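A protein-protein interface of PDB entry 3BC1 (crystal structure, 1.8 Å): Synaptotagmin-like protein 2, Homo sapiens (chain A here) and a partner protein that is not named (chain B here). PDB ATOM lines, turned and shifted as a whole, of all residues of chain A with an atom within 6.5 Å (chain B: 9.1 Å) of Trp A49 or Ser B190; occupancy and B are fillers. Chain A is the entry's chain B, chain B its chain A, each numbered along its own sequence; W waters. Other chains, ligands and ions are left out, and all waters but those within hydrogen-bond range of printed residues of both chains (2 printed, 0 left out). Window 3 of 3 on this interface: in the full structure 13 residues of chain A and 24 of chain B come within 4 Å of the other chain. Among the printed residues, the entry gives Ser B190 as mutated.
The backbone carbonyl oxygen (O) of Lys A43 is in hydrogen-bond range of the backbone NH (N) of Trp A49, 3.2 Å away. OH of Tyr B124 sits at hydrogen-bond distance from NE of Arg B186 (3.0 Å). OD1 of Asn A44 sits at hydrogen-bond distance from NE2 of Gln A40, 2.9 Å away. The backbone carbonyl oxygen (O) of Arg B186 sits at hydrogen-bond distance from the side-chain hydroxyl (OG) of Ser B190 (2.7 Å). O of Lys B13 sits at hydrogen-bond distance from N of Met B95, at 2.8 Å.
Asn A44 touches Tyr B10. Asn A44 touches Met B187 (CB to SD, 3.8 Å). Met A45 touches Asp B9. Met A45 touches Tyr B10. Trp A49 touches Ile B183 (CH2 to O, 3.9 Å). NE1 of Trp A49 touches CE of Met B187 (3.4 Å). Trp A49 touches Ser B190 (CE3 to OG, 3.7 Å). Ala B94 touches Phe A50 (O to CZ, 3.4 Å). CZ of Phe A50 touches CA of Met B95, at 3.7 Å. Tyr B124 touches Phe A50.
Lys A43 touches none of the printed residues of chain B. Trp A49 touches just these residues of chain B: Ile B183 (3.9 Å), Met B187 (3.4 Å) and Ser B190 (3.7 Å). Printed residues of chain B within 4 Å of Phe A50: Ala B94, Met B95 and Tyr B124. Printed residues of chain A within 4 Å of Asp B9: Met A45. Printed residues of chain A within 4 Å of Tyr B124: Phe A50. Leu B180 touches none of the printed residues of chain A. The nearest residue of chain B that does not touch Trp A49 is Arg B186 (4.03 Å).
Of the 23 printed residues of chain B, 8 touch a printed residue of chain A. Hydrophobic or aromatic side chains of chain B that line the printed part of chain A: Tyr B10, Met B95, Tyr B124 and Met B187. Of the 11 printed residues of chain A, 4 touch a printed residue of chain B. Printed residues of chain A that touch a printed residue of chain B: Asn A44, Met A45, Trp A49 and Phe A50. Among the printed residues, 10 pairs touch across the chains. Among the printed residues, no Asp or Glu carboxylate lies within 4 Å of a Lys or Arg side-chain nitrogen of the other chain.
Water W2 bridges the backbone carbonyl oxygen (O) of Met A45 (2.5 Å) and the backbone NH (N) of Leu B11 (2.9 Å). Water W1 lies within hydrogen-bond range of NE2 of Gln A40 (3.0 Å) and O of Ser B190 (3.2 Å).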
ATOM      1  N   GLN A  40     -13.179  16.427  35.903  1.00  0.00           N
ATOM      2  CA  GLN A  40     -13.064  16.955  34.536  1.00  0.00           C
ATOM      3  C   GLN A  40     -14.018  16.239  33.579  1.00  0.00           C
ATOM      4  O   GLN A  40     -14.632  16.876  32.721  1.00  0.00           O
ATOM      5  CB  GLN A  40     -11.629  16.843  34.012  1.00  0.00           C
ATOM      6  CG  GLN A  40     -11.434  17.371  32.583  1.00  0.00           C
ATOM      7  CD  GLN A  40     -11.770  18.849  32.451  1.00  0.00           C
ATOM      8  OE1 GLN A  40     -10.965  19.712  32.796  1.00  0.00           O
ATOM      9  NE2 GLN A  40     -12.965  19.144  31.948  1.00  0.00           N
ATOM     10  N   LYS A  43     -17.404  17.546  34.390  1.00  0.00           N
ATOM     11  CA  LYS A  43     -17.569  18.870  33.763  1.00  0.00           C
ATOM     12  C   LYS A  43     -17.929  18.762  32.287  1.00  0.00           C
ATOM     13  O   LYS A  43     -18.734  19.540  31.779  1.00  0.00           O
ATOM     14  CB  LYS A  43     -16.293  19.715  33.873  1.00  0.00           C
ATOM     15  CG  LYS A  43     -16.096  20.458  35.188  1.00  0.00           C
ATOM     16  CD  LYS A  43     -15.265  21.738  34.977  1.00  0.00           C
ATOM     17  CE  LYS A  43     -14.173  21.893  36.023  1.00  0.00           C
ATOM     18  NZ  LYS A  43     -13.036  20.954  35.773  1.00  0.00           N
ATOM     19  N   ASN A  44     -17.303  17.814  31.601  1.00  0.00           N
ATOM     20  CA  ASN A  44     -17.572  17.576  30.185  1.00  0.00           C
ATOM     21  C   ASN A  44     -18.972  17.013  29.968  1.00  0.00           C
ATOM     22  O   ASN A  44     -19.776  17.578  29.218  1.00  0.00           O
ATOM     23  CB  ASN A  44     -16.530  16.615  29.604  1.00  0.00           C
ATOM     24  CG  ASN A  44     -15.133  17.211  29.573  1.00  0.00           C
ATOM     25  OD1 ASN A  44     -14.923  18.364  29.947  1.00  0.00           O
ATOM     26  ND2 ASN A  44     -14.167  16.419  29.130  1.00  0.00           N
ATOM     27  N   MET A  45     -19.256  15.902  30.642  1.00  0.00           N
ATOM     28  CA  MET A  45     -20.532  15.210  30.498  1.00  0.00           C
ATOM     29  C   MET A  45     -21.718  16.058  30.963  1.00  0.00           C
ATOM     30  O   MET A  45     -22.798  15.971  30.385  1.00  0.00           O
ATOM     31  CB  MET A  45     -20.498  13.873  31.242  1.00  0.00           C
ATOM     32  CG  MET A  45     -19.572  12.845  30.595  1.00  0.00           C
ATOM     33  SD  MET A  45     -19.400  11.345  31.580  1.00  0.00           S
ATOM     34  CE  MET A  45     -18.834  10.191  30.333  1.00  0.00           C
ATOM     35  N   SER A  46     -21.511  16.882  31.987  1.00  0.00           N
ATOM     36  CA  SER A  46     -22.579  17.726  32.528  1.00  0.00           C
ATOM     37  C   SER A  46     -22.893  18.934  31.646  1.00  0.00           C
ATOM     38  O   SER A  46     -23.931  19.570  31.825  1.00  0.00           O
ATOM     39  CB  SER A  46     -22.204  18.230  33.924  1.00  0.00           C
ATOM     40  OG  SER A  46     -21.144  19.168  33.847  1.00  0.00           O
ATOM     41  N   GLY A  47     -21.991  19.268  30.726  1.00  0.00           N
ATOM     42  CA  GLY A  47     -22.138  20.456  29.887  1.00  0.00           C
ATOM     43  C   GLY A  47     -21.610  21.732  30.526  1.00  0.00           C
ATOM     44  O   GLY A  47     -21.673  22.800  29.922  1.00  0.00           O
ATOM     45  N   GLN A  48     -21.082  21.626  31.746  1.00  0.00           N
ATOM     46  CA  GLN A  48     -20.506  22.777  32.447  1.00  0.00           C
ATOM     47  C   GLN A  48     -19.342  23.412  31.678  1.00  0.00           C
ATOM     48  O   GLN A  48     -19.113  24.618  31.779  1.00  0.00           O
ATOM     49  CB  GLN A  48     -20.053  22.365  33.854  1.00  0.00           C
ATOM     50  CG  GLN A  48     -19.293  23.438  34.620  1.00  0.00           C
ATOM     51  CD  GLN A  48     -19.009  23.056  36.067  1.00  0.00           C
ATOM     52  OE1 GLN A  48     -17.952  23.395  36.609  1.00  0.00           O
ATOM     53  NE2 GLN A  48     -19.950  22.358  36.701  1.00  0.00           N
ATOM     54  N   TRP A  49     -18.617  22.599  30.911  1.00  0.00           N
ATOM     55  CA  TRP A  49     -17.516  23.087  30.075  1.00  0.00           C
ATOM     56  C   TRP A  49     -17.953  24.233  29.152  1.00  0.00           C
ATOM     57  O   TRP A  49     -17.167  25.134  28.862  1.00  0.00           O
ATOM     58  CB  TRP A  49     -16.932  21.940  29.231  1.00  0.00           C
ATOM     59  CG  TRP A  49     -17.816  21.528  28.087  1.00  0.00           C
ATOM     60  CD1 TRP A  49     -18.788  20.573  28.105  1.00  0.00           C
ATOM     61  CD2 TRP A  49     -17.817  22.076  26.760  1.00  0.00           C
ATOM     62  NE1 TRP A  49     -19.392  20.487  26.873  1.00  0.00           N
ATOM     63  CE2 TRP A  49     -18.815  21.400  26.030  1.00  0.00           C
ATOM     64  CE3 TRP A  49     -17.068  23.072  26.119  1.00  0.00           C
ATOM     65  CZ2 TRP A  49     -19.085  21.683  24.686  1.00  0.00           C
ATOM     66  CZ3 TRP A  49     -17.338  23.355  24.781  1.00  0.00           C
ATOM     67  CH2 TRP A  49     -18.337  22.661  24.083  1.00  0.00           C
ATOM     68  N   PHE A  50     -19.204  24.183  28.690  1.00  0.00           N
ATOM     69  CA  PHE A  50     -19.756  25.179  27.770  1.00  0.00           C
ATOM     70  C   PHE A  50     -19.931  26.551  28.430  1.00  0.00           C
ATOM     71  O   PHE A  50     -19.954  27.574  27.742  1.00  0.00           O
ATOM     72  CB  PHE A  50     -21.096  24.684  27.211  1.00  0.00           C
ATOM     73  CG  PHE A  50     -21.682  25.571  26.142  1.00  0.00           C
ATOM     74  CD1 PHE A  50     -20.968  25.849  24.983  1.00  0.00           C
ATOM     75  CD2 PHE A  50     -22.954  26.113  26.289  1.00  0.00           C
ATOM     76  CE1 PHE A  50     -21.505  26.661  23.997  1.00  0.00           C
ATOM     77  CE2 PHE A  50     -23.498  26.923  25.304  1.00  0.00           C
ATOM     78  CZ  PHE A  50     -22.771  27.197  24.157  1.00  0.00           C
ATOM     79  N   TYR A  51     -20.053  26.566  29.758  1.00  0.00           N
ATOM     80  CA  TYR A  51     -20.086  27.812  30.531  1.00  0.00           C
ATOM     81  C   TYR A  51     -18.727  28.115  31.181  1.00  0.00           C
ATOM     82  O   TYR A  51     -18.635  28.976  32.057  1.00  0.00           O
ATOM     83  CB  TYR A  51     -21.175  27.732  31.605  1.00  0.00           C
ATOM     84  CG  TYR A  51     -22.533  27.343  31.062  1.00  0.00           C
ATOM     85  CD1 TYR A  51     -22.949  26.013  31.061  1.00  0.00           C
ATOM     86  CD2 TYR A  51     -23.398  28.303  30.548  1.00  0.00           C
ATOM     87  CE1 TYR A  51     -24.193  25.648  30.563  1.00  0.00           C
ATOM     88  CE2 TYR A  51     -24.646  27.950  30.046  1.00  0.00           C
ATOM     89  CZ  TYR A  51     -25.038  26.621  30.055  1.00  0.00           C
ATOM     90  OH  TYR A  51     -26.272  26.268  29.554  1.00  0.00           O
ATOM     91  N   GLU A  52     -17.680  27.423  30.726  1.00  0.00           N
ATOM     92  CA  GLU A  52     -16.356  27.439  31.360  1.00  0.00           C
ATOM     93  C   GLU A  52     -16.417  26.986  32.817  1.00  0.00           C
ATOM     94  O   GLU A  52     -15.830  25.963  33.184  1.00  0.00           O
ATOM     95  CB  GLU A  52     -15.690  28.817  31.255  1.00  0.00           C
ATOM     96  CG  GLU A  52     -15.449  29.285  29.824  1.00  0.00           C
ATOM     97  CD  GLU A  52     -14.181  30.121  29.675  1.00  0.00           C
ATOM     98  OE1 GLU A  52     -13.875  30.930  30.580  1.00  0.00           O
ATOM     99  OE2 GLU A  52     -13.491  29.974  28.642  1.00  0.00           O
ATOM    100  N   ASP B   9     -24.315  10.060  27.292  1.00  0.00           N
ATOM    101  CA  ASP B   9     -23.154  10.666  27.947  1.00  0.00           C
ATOM    102  C   ASP B   9     -23.089  12.192  27.849  1.00  0.00           C
ATOM    103  O   ASP B   9     -22.588  12.840  28.773  1.00  0.00           O
ATOM    104  CB  ASP B   9     -21.870  10.066  27.366  1.00  0.00           C
ATOM    105  CG  ASP B   9     -21.795   8.563  27.552  1.00  0.00           C
ATOM    106  OD1 ASP B   9     -21.989   8.091  28.690  1.00  0.00           O
ATOM    107  OD2 ASP B   9     -21.554   7.851  26.557  1.00  0.00           O
ATOM    108  N   TYR B  10     -23.562  12.753  26.735  1.00  0.00           N
ATOM    109  CA  TYR B  10     -23.547  14.208  26.507  1.00  0.00           C
ATOM    110  C   TYR B  10     -24.839  14.689  25.853  1.00  0.00           C
ATOM    111  O   TYR B  10     -25.325  14.069  24.909  1.00  0.00           O
ATOM    112  CB  TYR B  10     -22.371  14.607  25.605  1.00  0.00           C
ATOM    113  CG  TYR B  10     -21.030  14.139  26.110  1.00  0.00           C
ATOM    114  CD1 TYR B  10     -20.271  14.933  26.958  1.00  0.00           C
ATOM    115  CD2 TYR B  10     -20.521  12.893  25.748  1.00  0.00           C
ATOM    116  CE1 TYR B  10     -19.043  14.502  27.437  1.00  0.00           C
ATOM    117  CE2 TYR B  10     -19.286  12.456  26.221  1.00  0.00           C
ATOM    118  CZ  TYR B  10     -18.559  13.266  27.066  1.00  0.00           C
ATOM    119  OH  TYR B  10     -17.340  12.852  27.548  1.00  0.00           O
ATOM    120  N   LEU B  11     -25.392  15.787  26.362  1.00  0.00           N
ATOM    121  CA  LEU B  11     -26.469  16.494  25.674  1.00  0.00           C
ATOM    122  C   LEU B  11     -25.824  17.634  24.899  1.00  0.00           C
ATOM    123  O   LEU B  11     -25.222  18.537  25.496  1.00  0.00           O
ATOM    124  CB  LEU B  11     -27.520  17.042  26.653  1.00  0.00           C
ATOM    125  CG  LEU B  11     -28.648  17.901  26.049  1.00  0.00           C
ATOM    126  CD1 LEU B  11     -29.426  17.126  25.011  1.00  0.00           C
ATOM    127  CD2 LEU B  11     -29.595  18.434  27.119  1.00  0.00           C
ATOM    128  N   ILE B  12     -25.942  17.576  23.574  1.00  0.00           N
ATOM    129  CA  ILE B  12     -25.390  18.592  22.688  1.00  0.00           C
ATOM    130  C   ILE B  12     -26.548  19.331  22.026  1.00  0.00           C
ATOM    131  O   ILE B  12     -27.463  18.704  21.504  1.00  0.00           O
ATOM    132  CB  ILE B  12     -24.484  17.974  21.615  1.00  0.00           C
ATOM    133  CG1 ILE B  12     -23.330  17.198  22.261  1.00  0.00           C
ATOM    134  CG2 ILE B  12     -23.938  19.051  20.700  1.00  0.00           C
ATOM    135  CD1 ILE B  12     -22.354  18.067  23.024  1.00  0.00           C
ATOM    136  N   LYS B  13     -26.513  20.660  22.079  1.00  0.00           N
ATOM    137  CA  LYS B  13     -27.602  21.493  21.563  1.00  0.00           C
ATOM    138  C   LYS B  13     -27.130  22.295  20.353  1.00  0.00           C
ATOM    139  O   LYS B  13     -26.153  23.044  20.443  1.00  0.00           O
ATOM    140  CB  LYS B  13     -28.128  22.439  22.655  1.00  0.00           C
ATOM    141  CG  LYS B  13     -28.556  21.736  23.947  1.00  0.00           C
ATOM    142  CD  LYS B  13     -29.092  22.712  24.991  1.00  0.00           C
ATOM    143  CE  LYS B  13     -29.387  21.997  26.310  1.00  0.00           C
ATOM    144  NZ  LYS B  13     -30.044  22.865  27.349  1.00  0.00           N
ATOM    145  N   PHE B  14     -27.812  22.120  19.221  1.00  0.00           N
ATOM    146  CA  PHE B  14     -27.547  22.910  18.018  1.00  0.00           C
ATOM    147  C   PHE B  14     -28.776  23.720  17.628  1.00  0.00           C
ATOM    148  O   PHE B  14     -29.890  23.418  18.052  1.00  0.00           O
ATOM    149  CB  PHE B  14     -27.148  22.023  16.830  1.00  0.00           C
ATOM    150  CG  PHE B  14     -25.821  21.319  16.997  1.00  0.00           C
ATOM    151  CD1 PHE B  14     -24.767  21.921  17.673  1.00  0.00           C
ATOM    152  CD2 PHE B  14     -25.621  20.068  16.436  1.00  0.00           C
ATOM    153  CE1 PHE B  14     -23.547  21.271  17.816  1.00  0.00           C
ATOM    154  CE2 PHE B  14     -24.398  19.415  16.570  1.00  0.00           C
ATOM    155  CZ  PHE B  14     -23.365  20.027  17.261  1.00  0.00           C
ATOM    156  N   ALA B  94     -27.212  27.933  22.252  1.00  0.00           N
ATOM    157  CA  ALA B  94     -26.809  26.907  21.282  1.00  0.00           C
ATOM    158  C   ALA B  94     -25.288  26.719  21.245  1.00  0.00           C
ATOM    159  O   ALA B  94     -24.539  27.689  21.251  1.00  0.00           O
ATOM    160  CB  ALA B  94     -27.326  27.261  19.900  1.00  0.00           C
ATOM    161  N   MET B  95     -24.843  25.466  21.169  1.00  0.00           N
ATOM    162  CA  MET B  95     -23.410  25.142  21.135  1.00  0.00           C
ATOM    163  C   MET B  95     -22.797  25.251  19.738  1.00  0.00           C
ATOM    164  O   MET B  95     -21.581  25.355  19.591  1.00  0.00           O
ATOM    165  CB  MET B  95     -23.177  23.739  21.673  1.00  0.00           C
ATOM    166  CG  MET B  95     -23.664  23.539  23.082  1.00  0.00           C
ATOM    167  SD  MET B  95     -23.491  21.825  23.572  1.00  0.00           S
ATOM    168  CE  MET B  95     -24.035  21.907  25.270  1.00  0.00           C
ATOM    169  N   GLY B  96     -23.644  25.238  18.716  1.00  0.00           N
ATOM    170  CA  GLY B  96     -23.193  25.324  17.340  1.00  0.00           C
ATOM    171  C   GLY B  96     -24.379  25.623  16.459  1.00  0.00           C
ATOM    172  O   GLY B  96     -25.518  25.432  16.875  1.00  0.00           O
ATOM    173  N   TYR B 124     -22.864  32.437  22.151  1.00  0.00           N
ATOM    174  CA  TYR B 124     -22.028  32.271  23.351  1.00  0.00           C
ATOM    175  C   TYR B 124     -20.605  32.801  23.127  1.00  0.00           C
ATOM    176  O   TYR B 124     -19.931  33.210  24.075  1.00  0.00           O
ATOM    177  CB  TYR B 124     -21.967  30.798  23.773  1.00  0.00           C
ATOM    178  CG  TYR B 124     -20.993  29.970  22.960  1.00  0.00           C
ATOM    179  CD1 TYR B 124     -19.691  29.748  23.411  1.00  0.00           C
ATOM    180  CD2 TYR B 124     -21.361  29.427  21.733  1.00  0.00           C
ATOM    181  CE1 TYR B 124     -18.792  28.999  22.665  1.00  0.00           C
ATOM    182  CE2 TYR B 124     -20.471  28.676  20.979  1.00  0.00           C
ATOM    183  CZ  TYR B 124     -19.188  28.466  21.448  1.00  0.00           C
ATOM    184  OH  TYR B 124     -18.299  27.719  20.705  1.00  0.00           O
ATOM    185  N   ASP B 129     -19.010  27.888  16.296  1.00  0.00           N
ATOM    186  CA  ASP B 129     -18.965  26.893  15.228  1.00  0.00           C
ATOM    187  C   ASP B 129     -20.241  26.985  14.396  1.00  0.00           C
ATOM    188  O   ASP B 129     -21.350  26.947  14.936  1.00  0.00           O
ATOM    189  CB  ASP B 129     -18.796  25.484  15.802  1.00  0.00           C
ATOM    190  CG  ASP B 129     -17.466  25.303  16.513  1.00  0.00           C
ATOM    191  OD1 ASP B 129     -16.421  25.605  15.900  1.00  0.00           O
ATOM    192  OD2 ASP B 129     -17.467  24.863  17.681  1.00  0.00           O
ATOM    193  N   LEU B 179     -20.639  19.408  12.338  1.00  0.00           N
ATOM    194  CA  LEU B 179     -20.927  20.328  13.429  1.00  0.00           C
ATOM    195  C   LEU B 179     -20.711  19.652  14.781  1.00  0.00           C
ATOM    196  O   LEU B 179     -20.171  20.268  15.696  1.00  0.00           O
ATOM    197  CB  LEU B 179     -22.358  20.865  13.310  1.00  0.00           C
ATOM    198  CG  LEU B 179     -22.755  22.033  14.214  1.00  0.00           C
ATOM    199  CD1 LEU B 179     -21.745  23.174  14.126  1.00  0.00           C
ATOM    200  CD2 LEU B 179     -24.149  22.530  13.849  1.00  0.00           C
ATOM    201  N   LEU B 180     -21.112  18.387  14.896  1.00  0.00           N
ATOM    202  CA  LEU B 180     -20.859  17.606  16.112  1.00  0.00           C
ATOM    203  C   LEU B 180     -19.357  17.434  16.373  1.00  0.00           C
ATOM    204  O   LEU B 180     -18.898  17.583  17.504  1.00  0.00           O
ATOM    205  CB  LEU B 180     -21.551  16.237  16.042  1.00  0.00           C
ATOM    206  CG  LEU B 180     -21.393  15.346  17.277  1.00  0.00           C
ATOM    207  CD1 LEU B 180     -21.846  16.073  18.535  1.00  0.00           C
ATOM    208  CD2 LEU B 180     -22.151  14.039  17.110  1.00  0.00           C
ATOM    209  N   ASP B 181     -18.597  17.133  15.323  1.00  0.00           N
ATOM    210  CA  ASP B 181     -17.150  16.961  15.449  1.00  0.00           C
ATOM    211  C   ASP B 181     -16.482  18.250  15.939  1.00  0.00           C
ATOM    212  O   ASP B 181     -15.618  18.216  16.823  1.00  0.00           O
ATOM    213  CB  ASP B 181     -16.544  16.531  14.113  1.00  0.00           C
ATOM    214  CG  ASP B 181     -15.108  16.061  14.249  1.00  0.00           C
ATOM    215  OD1 ASP B 181     -14.838  15.194  15.113  1.00  0.00           O
ATOM    216  OD2 ASP B 181     -14.253  16.562  13.500  1.00  0.00           O
ATOM    217  N   LEU B 182     -16.902  19.381  15.375  1.00  0.00           N
ATOM    218  CA  LEU B 182     -16.375  20.686  15.778  1.00  0.00           C
ATOM    219  C   LEU B 182     -16.608  20.994  17.259  1.00  0.00           C
ATOM    220  O   LEU B 182     -15.719  21.521  17.929  1.00  0.00           O
ATOM    221  CB  LEU B 182     -16.981  21.800  14.913  1.00  0.00           C
ATOM    222  CG  LEU B 182     -16.563  21.793  13.443  1.00  0.00           C
ATOM    223  CD1 LEU B 182     -17.356  22.832  12.651  1.00  0.00           C
ATOM    224  CD2 LEU B 182     -15.065  22.035  13.313  1.00  0.00           C
ATOM    225  N   ILE B 183     -17.785  20.671  17.787  1.00  0.00           N
ATOM    226  CA  ILE B 183     -18.056  21.017  19.188  1.00  0.00           C
ATOM    227  C   ILE B 183     -17.396  20.033  20.165  1.00  0.00           C
ATOM    228  O   ILE B 183     -16.966  20.437  21.250  1.00  0.00           O
ATOM    229  CB  ILE B 183     -19.573  21.237  19.484  1.00  0.00           C
ATOM    230  CG1 ILE B 183     -20.286  19.929  19.820  1.00  0.00           C
ATOM    231  CG2 ILE B 183     -20.242  22.010  18.330  1.00  0.00           C
ATOM    232  CD1 ILE B 183     -20.190  19.574  21.285  1.00  0.00           C
ATOM    233  N   MET B 184     -17.293  18.760  19.773  1.00  0.00           N
ATOM    234  CA  MET B 184     -16.616  17.760  20.603  1.00  0.00           C
ATOM    235  C   MET B 184     -15.109  18.036  20.677  1.00  0.00           C
ATOM    236  O   MET B 184     -14.482  17.792  21.708  1.00  0.00           O
ATOM    237  CB  MET B 184     -16.871  16.335  20.086  1.00  0.00           C
ATOM    238  CG  MET B 184     -18.335  15.877  20.145  1.00  0.00           C
ATOM    239  SD  MET B 184     -19.053  15.816  21.795  1.00  0.00           S
ATOM    240  CE  MET B 184     -18.199  14.412  22.506  1.00  0.00           C
ATOM    241  N   LYS B 185     -14.535  18.542  19.583  1.00  0.00           N
ATOM    242  CA  LYS B 185     -13.134  18.967  19.576  1.00  0.00           C
ATOM    243  C   LYS B 185     -12.915  20.237  20.395  1.00  0.00           C
ATOM    244  O   LYS B 185     -11.873  20.397  21.033  1.00  0.00           O
ATOM    245  CB  LYS B 185     -12.634  19.174  18.150  1.00  0.00           C
ATOM    246  CG  LYS B 185     -12.365  17.878  17.430  1.00  0.00           C
ATOM    247  CD  LYS B 185     -11.886  18.116  16.011  1.00  0.00           C
ATOM    248  CE  LYS B 185     -11.218  16.864  15.445  1.00  0.00           C
ATOM    249  NZ  LYS B 185     -12.045  15.636  15.633  1.00  0.00           N
ATOM    250  N   ARG B 186     -13.891  21.141  20.365  1.00  0.00           N
ATOM    251  CA  ARG B 186     -13.867  22.322  21.224  1.00  0.00           C
ATOM    252  C   ARG B 186     -13.896  21.913  22.699  1.00  0.00           C
ATOM    253  O   ARG B 186     -13.197  22.502  23.526  1.00  0.00           O
ATOM    254  CB  ARG B 186     -15.048  23.237  20.902  1.00  0.00           C
ATOM    255  CG  ARG B 186     -15.055  24.542  21.678  1.00  0.00           C
ATOM    256  CD  ARG B 186     -16.220  25.409  21.254  1.00  0.00           C
ATOM    257  NE  ARG B 186     -16.002  25.996  19.933  1.00  0.00           N
ATOM    258  CZ  ARG B 186     -15.496  27.208  19.706  1.00  0.00           C
ATOM    259  NH1 ARG B 186     -15.126  28.003  20.707  1.00  0.00           N
ATOM    260  NH2 ARG B 186     -15.358  27.633  18.456  1.00  0.00           N
ATOM    261  N   MET B 187     -14.708  20.907  23.021  1.00  0.00           N
ATOM    262  CA  MET B 187     -14.748  20.350  24.374  1.00  0.00           C
ATOM    263  C   MET B 187     -13.379  19.781  24.743  1.00  0.00           C
ATOM    264  O   MET B 187     -12.902  19.984  25.860  1.00  0.00           O
ATOM    265  CB  MET B 187     -15.824  19.258  24.479  1.00  0.00           C
ATOM    266  CG  MET B 187     -15.976  18.642  25.866  1.00  0.00           C
ATOM    267  SD  MET B 187     -16.912  17.095  25.857  1.00  0.00           S
ATOM    268  CE  MET B 187     -18.494  17.668  25.233  1.00  0.00           C
ATOM    269  N   GLU B 188     -12.759  19.070  23.800  1.00  0.00           N
ATOM    270  CA  GLU B 188     -11.407  18.520  23.982  1.00  0.00           C
ATOM    271  C   GLU B 188     -10.377  19.632  24.189  1.00  0.00           C
ATOM    272  O   GLU B 188      -9.585  19.575  25.132  1.00  0.00           O
ATOM    273  CB  GLU B 188     -11.007  17.657  22.776  1.00  0.00           C
ATOM    274  CG  GLU B 188     -11.557  16.227  22.802  1.00  0.00           C
ATOM    275  CD  GLU B 188     -10.644  15.232  23.521  1.00  0.00           C
ATOM    276  OE1 GLU B 188      -9.398  15.360  23.428  1.00  0.00           O
ATOM    277  OE2 GLU B 188     -11.180  14.304  24.168  1.00  0.00           O
ATOM    278  N   ARG B 189     -10.393  20.624  23.297  1.00  0.00           N
ATOM    279  CA  ARG B 189      -9.578  21.841  23.435  1.00  0.00           C
ATOM    280  C   ARG B 189      -9.660  22.426  24.845  1.00  0.00           C
ATOM    281  O   ARG B 189      -8.635  22.678  25.474  1.00  0.00           O
ATOM    282  CB  ARG B 189     -10.036  22.921  22.440  1.00  0.00           C
ATOM    283  CG  ARG B 189      -9.193  23.069  21.174  1.00  0.00           C
ATOM    284  CD  ARG B 189      -9.876  24.017  20.178  1.00  0.00           C
ATOM    285  NE  ARG B 189     -10.620  23.293  19.141  1.00  0.00           N
ATOM    286  CZ  ARG B 189     -11.683  23.754  18.477  1.00  0.00           C
ATOM    287  NH1 ARG B 189     -12.195  24.957  18.731  1.00  0.00           N
ATOM    288  NH2 ARG B 189     -12.256  22.988  17.551  1.00  0.00           N
ATOM    289  N   SER B 190     -10.882  22.654  25.324  1.00  0.00           N
ATOM    290  CA  SER B 190     -11.100  23.289  26.627  1.00  0.00           C
ATOM    291  C   SER B 190     -11.328  22.256  27.722  1.00  0.00           C
ATOM    292  O   SER B 190     -10.593  22.221  28.711  1.00  0.00           O
ATOM    293  CB  SER B 190     -12.279  24.268  26.565  1.00  0.00           C
ATOM    294  OG  SER B 190     -13.424  23.681  25.969  1.00  0.00           O
HETATM  295  O   HOH W   1     -13.081  21.856  30.650  1.00  0.00           O
HETATM  296  O   HOH W   2     -24.098  17.181  28.582  1.00  0.00           O
